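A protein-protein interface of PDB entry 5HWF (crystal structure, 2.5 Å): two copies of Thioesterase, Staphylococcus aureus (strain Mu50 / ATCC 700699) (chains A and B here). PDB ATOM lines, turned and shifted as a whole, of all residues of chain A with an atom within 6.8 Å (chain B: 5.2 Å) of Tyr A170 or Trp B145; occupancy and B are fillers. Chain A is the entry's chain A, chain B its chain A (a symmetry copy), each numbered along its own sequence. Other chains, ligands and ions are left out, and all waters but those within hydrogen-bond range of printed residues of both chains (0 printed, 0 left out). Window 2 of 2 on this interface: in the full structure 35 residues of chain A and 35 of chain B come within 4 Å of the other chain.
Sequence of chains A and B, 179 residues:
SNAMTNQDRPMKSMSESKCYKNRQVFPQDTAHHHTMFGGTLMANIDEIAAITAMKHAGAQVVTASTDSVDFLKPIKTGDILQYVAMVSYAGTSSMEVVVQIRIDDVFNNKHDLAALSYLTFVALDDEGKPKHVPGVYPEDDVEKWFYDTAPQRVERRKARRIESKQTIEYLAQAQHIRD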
ATOM      1  N   GLU A 163     -19.239  11.109 -18.830  1.00  0.00           N
ATOM      2  CA  GLU A 163     -19.168  11.957 -20.027  1.00  0.00           C
ATOM      3  C   GLU A 163     -19.198  11.137 -21.323  1.00  0.00           C
ATOM      4  O   GLU A 163     -19.901  11.468 -22.293  1.00  0.00           O
ATOM      5  CB  GLU A 163     -17.909  12.827 -19.986  1.00  0.00           C
ATOM      6  CG  GLU A 163     -17.897  13.849 -18.848  1.00  0.00           C
ATOM      7  CD  GLU A 163     -19.089  14.801 -18.892  1.00  0.00           C
ATOM      8  OE1 GLU A 163     -19.489  15.218 -20.002  1.00  0.00           O
ATOM      9  OE2 GLU A 163     -19.632  15.134 -17.816  1.00  0.00           O
ATOM     10  N   LYS A 165     -20.413   8.180 -21.808  1.00  0.00           N
ATOM     11  CA  LYS A 165     -21.767   7.683 -22.058  1.00  0.00           C
ATOM     12  C   LYS A 165     -22.641   8.755 -22.718  1.00  0.00           C
ATOM     13  O   LYS A 165     -23.443   8.458 -23.623  1.00  0.00           O
ATOM     14  CB  LYS A 165     -22.415   7.189 -20.765  1.00  0.00           C
ATOM     15  CG  LYS A 165     -22.519   5.661 -20.673  1.00  0.00           C
ATOM     16  CD  LYS A 165     -23.202   5.049 -21.906  1.00  0.00           C
ATOM     17  CE  LYS A 165     -23.701   3.622 -21.638  1.00  0.00           C
ATOM     18  NZ  LYS A 165     -24.510   3.078 -22.768  1.00  0.00           N
ATOM     19  N   GLN A 166     -22.480  10.003 -22.280  1.00  0.00           N
ATOM     20  CA  GLN A 166     -23.190  11.107 -22.935  1.00  0.00           C
ATOM     21  C   GLN A 166     -22.871  11.211 -24.427  1.00  0.00           C
ATOM     22  O   GLN A 166     -23.768  11.399 -25.270  1.00  0.00           O
ATOM     23  CB  GLN A 166     -22.841  12.425 -22.268  1.00  0.00           C
ATOM     24  CG  GLN A 166     -24.006  13.206 -21.762  1.00  0.00           C
ATOM     25  CD  GLN A 166     -23.553  14.191 -20.728  1.00  0.00           C
ATOM     26  OE1 GLN A 166     -23.849  14.047 -19.538  1.00  0.00           O
ATOM     27  NE2 GLN A 166     -22.788  15.185 -21.163  1.00  0.00           N
ATOM     28  N   THR A 167     -21.580  11.110 -24.743  1.00  0.00           N
ATOM     29  CA  THR A 167     -21.136  11.168 -26.134  1.00  0.00           C
ATOM     30  C   THR A 167     -21.713  10.038 -26.982  1.00  0.00           C
ATOM     31  O   THR A 167     -22.236  10.270 -28.086  1.00  0.00           O
ATOM     32  CB  THR A 167     -19.610  11.124 -26.232  1.00  0.00           C
ATOM     33  OG1 THR A 167     -19.074  12.338 -25.702  1.00  0.00           O
ATOM     34  CG2 THR A 167     -19.171  10.978 -27.689  1.00  0.00           C
ATOM     35  N   ILE A 168     -21.603   8.816 -26.467  1.00  0.00           N
ATOM     36  CA  ILE A 168     -22.173   7.650 -27.134  1.00  0.00           C
ATOM     37  C   ILE A 168     -23.643   7.883 -27.446  1.00  0.00           C
ATOM     38  O   ILE A 168     -24.092   7.663 -28.578  1.00  0.00           O
ATOM     39  CB  ILE A 168     -22.040   6.374 -26.273  1.00  0.00           C
ATOM     40  CG1 ILE A 168     -20.570   6.065 -25.980  1.00  0.00           C
ATOM     41  CG2 ILE A 168     -22.710   5.194 -26.962  1.00  0.00           C
ATOM     42  CD1 ILE A 168     -20.373   5.082 -24.826  1.00  0.00           C
ATOM     43  N   GLU A 169     -24.387   8.353 -26.447  1.00  0.00           N
ATOM     44  CA  GLU A 169     -25.822   8.566 -26.631  1.00  0.00           C
ATOM     45  C   GLU A 169     -26.118   9.645 -27.658  1.00  0.00           C
ATOM     46  O   GLU A 169     -27.071   9.511 -28.425  1.00  0.00           O
ATOM     47  CB  GLU A 169     -26.495   8.903 -25.306  1.00  0.00           C
ATOM     48  CG  GLU A 169     -26.700   7.663 -24.449  1.00  0.00           C
ATOM     49  CD  GLU A 169     -27.583   7.898 -23.242  1.00  0.00           C
ATOM     50  OE1 GLU A 169     -28.365   8.879 -23.245  1.00  0.00           O
ATOM     51  OE2 GLU A 169     -27.498   7.088 -22.292  1.00  0.00           O
ATOM     52  N   TYR A 170     -25.309  10.703 -27.692  1.00  0.00           N
ATOM     53  CA  TYR A 170     -25.471  11.690 -28.760  1.00  0.00           C
ATOM     54  C   TYR A 170     -25.224  11.095 -30.150  1.00  0.00           C
ATOM     55  O   TYR A 170     -26.027  11.294 -31.054  1.00  0.00           O
ATOM     56  CB  TYR A 170     -24.549  12.894 -28.584  1.00  0.00           C
ATOM     57  CG  TYR A 170     -24.841  13.940 -29.628  1.00  0.00           C
ATOM     58  CD1 TYR A 170     -25.908  14.820 -29.462  1.00  0.00           C
ATOM     59  CD2 TYR A 170     -24.089  14.031 -30.801  1.00  0.00           C
ATOM     60  CE1 TYR A 170     -26.213  15.769 -30.422  1.00  0.00           C
ATOM     61  CE2 TYR A 170     -24.389  14.998 -31.774  1.00  0.00           C
ATOM     62  CZ  TYR A 170     -25.454  15.860 -31.572  1.00  0.00           C
ATOM     63  OH  TYR A 170     -25.781  16.824 -32.503  1.00  0.00           O
ATOM     64  N   LEU A 171     -24.115  10.384 -30.327  1.00  0.00           N
ATOM     65  CA  LEU A 171     -23.814   9.797 -31.635  1.00  0.00           C
ATOM     66  C   LEU A 171     -24.908   8.840 -32.073  1.00  0.00           C
ATOM     67  O   LEU A 171     -25.247   8.783 -33.250  1.00  0.00           O
ATOM     68  CB  LEU A 171     -22.481   9.062 -31.620  1.00  0.00           C
ATOM     69  CG  LEU A 171     -21.268   9.936 -31.341  1.00  0.00           C
ATOM     70  CD1 LEU A 171     -20.033   9.061 -31.140  1.00  0.00           C
ATOM     71  CD2 LEU A 171     -21.068  10.933 -32.463  1.00  0.00           C
ATOM     72  N   ALA A 172     -25.455   8.096 -31.116  1.00  0.00           N
ATOM     73  CA  ALA A 172     -26.503   7.123 -31.398  1.00  0.00           C
ATOM     74  C   ALA A 172     -27.692   7.765 -32.116  1.00  0.00           C
ATOM     75  O   ALA A 172     -28.298   7.150 -32.992  1.00  0.00           O
ATOM     76  CB  ALA A 172     -26.956   6.457 -30.117  1.00  0.00           C
ATOM     77  N   GLN A 173     -28.025   8.999 -31.760  1.00  0.00           N
ATOM     78  CA  GLN A 173     -29.082   9.697 -32.471  1.00  0.00           C
ATOM     79  C   GLN A 173     -28.503  10.678 -33.495  1.00  0.00           C
ATOM     80  O   GLN A 173     -28.683  11.890 -33.391  1.00  0.00           O
ATOM     81  CB  GLN A 173     -30.017  10.411 -31.487  1.00  0.00           C
ATOM     82  CG  GLN A 173     -29.358  11.438 -30.589  1.00  0.00           C
ATOM     83  CD  GLN A 173     -30.346  12.480 -30.124  1.00  0.00           C
ATOM     84  OE1 GLN A 173     -31.238  12.200 -29.322  1.00  0.00           O
ATOM     85  NE2 GLN A 173     -30.226  13.687 -30.670  1.00  0.00           N
ATOM     86  N   ALA A 174     -27.812  10.141 -34.496  1.00  0.00           N
ATOM     87  CA  ALA A 174     -27.315  10.952 -35.608  1.00  0.00           C
ATOM     88  C   ALA A 174     -26.836  10.094 -36.785  1.00  0.00           C
ATOM     89  O   ALA A 174     -27.423   9.056 -37.104  1.00  0.00           O
ATOM     90  CB  ALA A 174     -26.193  11.865 -35.133  1.00  0.00           C
ATOM     91  N   ASP B 141     -23.291  18.374 -37.150  1.00  0.00           N
ATOM     92  CA  ASP B 141     -23.701  18.289 -35.739  1.00  0.00           C
ATOM     93  C   ASP B 141     -22.753  17.488 -34.845  1.00  0.00           C
ATOM     94  O   ASP B 141     -22.493  17.874 -33.703  1.00  0.00           O
ATOM     95  CB  ASP B 141     -25.099  17.676 -35.630  1.00  0.00           C
ATOM     96  CG  ASP B 141     -26.202  18.673 -35.911  1.00  0.00           C
ATOM     97  OD1 ASP B 141     -25.938  19.893 -35.866  1.00  0.00           O
ATOM     98  OD2 ASP B 141     -27.342  18.229 -36.167  1.00  0.00           O
ATOM     99  N   VAL B 142     -22.275  16.361 -35.368  1.00  0.00           N
ATOM    100  CA  VAL B 142     -21.319  15.502 -34.677  1.00  0.00           C
ATOM    101  C   VAL B 142     -20.029  16.271 -34.406  1.00  0.00           C
ATOM    102  O   VAL B 142     -19.502  16.274 -33.276  1.00  0.00           O
ATOM    103  CB  VAL B 142     -21.032  14.229 -35.506  1.00  0.00           C
ATOM    104  CG1 VAL B 142     -19.827  13.462 -34.958  1.00  0.00           C
ATOM    105  CG2 VAL B 142     -22.269  13.343 -35.552  1.00  0.00           C
ATOM    106  N   GLU B 143     -19.547  16.946 -35.448  1.00  0.00           N
ATOM    107  CA  GLU B 143     -18.329  17.736 -35.362  1.00  0.00           C
ATOM    108  C   GLU B 143     -18.438  18.765 -34.255  1.00  0.00           C
ATOM    109  O   GLU B 143     -17.508  18.945 -33.477  1.00  0.00           O
ATOM    110  CB  GLU B 143     -18.032  18.426 -36.691  1.00  0.00           C
ATOM    111  CG  GLU B 143     -17.590  17.473 -37.797  1.00  0.00           C
ATOM    112  CD  GLU B 143     -17.218  18.196 -39.090  1.00  0.00           C
ATOM    113  OE1 GLU B 143     -17.171  19.448 -39.094  1.00  0.00           O
ATOM    114  OE2 GLU B 143     -16.984  17.510 -40.107  1.00  0.00           O
ATOM    115  N   LYS B 144     -19.580  19.428 -34.165  1.00  0.00           N
ATOM    116  CA  LYS B 144     -19.713  20.460 -33.161  1.00  0.00           C
ATOM    117  C   LYS B 144     -19.993  19.848 -31.774  1.00  0.00           C
ATOM    118  O   LYS B 144     -19.735  20.486 -30.763  1.00  0.00           O
ATOM    119  CB  LYS B 144     -20.786  21.475 -33.572  1.00  0.00           C
ATOM    120  CG  LYS B 144     -22.195  21.196 -33.116  1.00  0.00           C
ATOM    121  CD  LYS B 144     -23.002  22.507 -33.095  1.00  0.00           C
ATOM    122  CE  LYS B 144     -22.627  23.363 -31.880  1.00  0.00           C
ATOM    123  NZ  LYS B 144     -23.516  24.520 -31.588  1.00  0.00           N
ATOM    124  N   TRP B 145     -20.477  18.608 -31.716  1.00  0.00           N
ATOM    125  CA  TRP B 145     -20.598  17.944 -30.423  1.00  0.00           C
ATOM    126  C   TRP B 145     -19.207  17.702 -29.830  1.00  0.00           C
ATOM    127  O   TRP B 145     -18.959  17.978 -28.642  1.00  0.00           O
ATOM    128  CB  TRP B 145     -21.345  16.612 -30.527  1.00  0.00           C
ATOM    129  CG  TRP B 145     -21.225  15.820 -29.241  1.00  0.00           C
ATOM    130  CD1 TRP B 145     -20.251  14.903 -28.920  1.00  0.00           C
ATOM    131  CD2 TRP B 145     -22.081  15.912 -28.096  1.00  0.00           C
ATOM    132  NE1 TRP B 145     -20.460  14.417 -27.647  1.00  0.00           N
ATOM    133  CE2 TRP B 145     -21.570  15.015 -27.121  1.00  0.00           C
ATOM    134  CE3 TRP B 145     -23.231  16.656 -27.801  1.00  0.00           C
ATOM    135  CZ2 TRP B 145     -22.177  14.844 -25.881  1.00  0.00           C
ATOM    136  CZ3 TRP B 145     -23.831  16.485 -26.569  1.00  0.00           C
ATOM    137  CH2 TRP B 145     -23.301  15.582 -25.620  1.00  0.00           C
ATOM    138  N   PHE B 146     -18.313  17.161 -30.662  1.00  0.00           N
ATOM    139  CA  PHE B 146     -16.936  16.927 -30.229  1.00  0.00           C
ATOM    140  C   PHE B 146     -16.189  18.240 -30.019  1.00  0.00           C
ATOM    141  O   PHE B 146     -15.305  18.341 -29.172  1.00  0.00           O
ATOM    142  CB  PHE B 146     -16.206  16.044 -31.244  1.00  0.00           C
ATOM    143  CG  PHE B 146     -16.653  14.613 -31.207  1.00  0.00           C
ATOM    144  CD1 PHE B 146     -16.434  13.838 -30.071  1.00  0.00           C
ATOM    145  CD2 PHE B 146     -17.318  14.046 -32.281  1.00  0.00           C
ATOM    146  CE1 PHE B 146     -16.856  12.522 -30.016  1.00  0.00           C
ATOM    147  CE2 PHE B 146     -17.741  12.725 -32.231  1.00  0.00           C
ATOM    148  CZ  PHE B 146     -17.504  11.959 -31.098  1.00  0.00           C
ATOM    149  N   TYR B 147     -16.558  19.254 -30.789  1.00  0.00           N
ATOM    150  CA  TYR B 147     -15.916  20.550 -30.674  1.00  0.00           C
ATOM    151  C   TYR B 147     -16.305  21.219 -29.359  1.00  0.00           C
ATOM    152  O   TYR B 147     -15.445  21.735 -28.644  1.00  0.00           O
ATOM    153  CB  TYR B 147     -16.286  21.437 -31.858  1.00  0.00           C
ATOM    154  CG  TYR B 147     -15.658  22.800 -31.798  1.00  0.00           C
ATOM    155  CD1 TYR B 147     -16.368  23.887 -31.320  1.00  0.00           C
ATOM    156  CD2 TYR B 147     -14.345  22.999 -32.208  1.00  0.00           C
ATOM    157  CE1 TYR B 147     -15.799  25.141 -31.260  1.00  0.00           C
ATOM    158  CE2 TYR B 147     -13.763  24.252 -32.145  1.00  0.00           C
ATOM    159  CZ  TYR B 147     -14.494  25.318 -31.666  1.00  0.00           C
ATOM    160  OH  TYR B 147     -13.933  26.573 -31.607  1.00  0.00           O
ATOM    161  N   ASP B 148     -17.601  21.175 -29.049  1.00  0.00           N
ATOM    162  CA  ASP B 148     -18.182  21.783 -27.849  1.00  0.00           C
ATOM    163  C   ASP B 148     -17.785  21.102 -26.551  1.00  0.00           C
ATOM    164  O   ASP B 148     -17.730  21.749 -25.517  1.00  0.00           O
ATOM    165  CB  ASP B 148     -19.711  21.778 -27.913  1.00  0.00           C
ATOM    166  CG  ASP B 148     -20.267  22.724 -28.953  1.00  0.00           C
ATOM    167  OD1 ASP B 148     -19.614  23.740 -29.279  1.00  0.00           O
ATOM    168  OD2 ASP B 148     -21.374  22.437 -29.439  1.00  0.00           O
ATOM    169  N   THR B 149     -17.539  19.800 -26.584  1.00  0.00           N
ATOM    170  CA  THR B 149     -17.237  19.090 -25.344  1.00  0.00           C
ATOM    171  C   THR B 149     -15.725  18.997 -25.086  1.00  0.00           C
ATOM    172  O   THR B 149     -15.294  18.543 -24.026  1.00  0.00           O
ATOM    173  CB  THR B 149     -17.870  17.675 -25.336  1.00  0.00           C
ATOM    174  OG1 THR B 149     -17.514  16.979 -26.533  1.00  0.00           O
ATOM    175  CG2 THR B 149     -19.388  17.770 -25.257  1.00  0.00           C
ATOM    176  N   ALA B 150     -14.927  19.463 -26.045  1.00  0.00           N
ATOM    177  CA  ALA B 150     -13.466  19.390 -25.952  1.00  0.00           C
ATOM    178  C   ALA B 150     -12.826  20.232 -24.823  1.00  0.00           C
ATOM    179  O   ALA B 150     -11.924  19.737 -24.153  1.00  0.00           O
ATOM    180  CB  ALA B 150     -12.834  19.765 -27.305  1.00  0.00           C
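Of chain B, only Asp B141 (3.3 Å) and Trp B145 (3.6 Å) come within 4 Å of Tyr A170. Trp B145 touches three residues of chain A. Printed residues of chain A within 4 Å of Phe B146: Thr A167 (3.6 Å) and Leu A171 (3.8 Å). Of the printed residues of chain B, Thr A167 touches Trp B145 and Phe B146. Printed residues of chain A within 4 Å of Val B142: Leu A171 (3.8 Å). Of the printed residues of chain A, Asp B141 touches Tyr A170. Of the printed residues of chain B, Gln A166 touches Trp B145. The nearest residue of chain B that does not touch Tyr A170 is Val B142 (4.3 Å).
The side-chain carboxylate (OE1) of Glu A163 is in hydrogen-bond range of the side-chain amide nitrogen (NE2) of Gln A166. The side-chain hydroxyl (OG1) of Thr B149 lies within hydrogen-bond range of the backbone carbonyl oxygen (O) of Trp B145 (2.7 Å).
Among the printed residues, merely in contact across the chains: Tyr A170 with Asp B141, Thr A167 with Phe B146, Tyr A170 with Trp B145, Leu A171 with Val B142, Leu A171 with Phe B146 and Gln A166 with Trp B145.
The indole nitrogen (NE1) of Trp B145 sits at hydrogen-bond distance from the side-chain hydroxyl (OG1) of Thr A167 (3.2 Å).
No position is printed for both chains. Of the 7 pairs that touch across the chains among the printed residues, none has its exchanged pair printed and touching as well.
Of the 10 printed residues of chain B, 4 touch a printed residue of chain A. Printed residues of chain B that touch a printed residue of chain A: Asp B141, Val B142, Trp B145 and Phe B146. Hydrophobic or aromatic side chains of chain B that line the printed part of chain A: Val B142, Trp B145 and Phe B146. Among the printed residues, no Asp or Glu carboxylate lies within 4 Å of a Lys or Arg side-chain nitrogen of the other chain.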
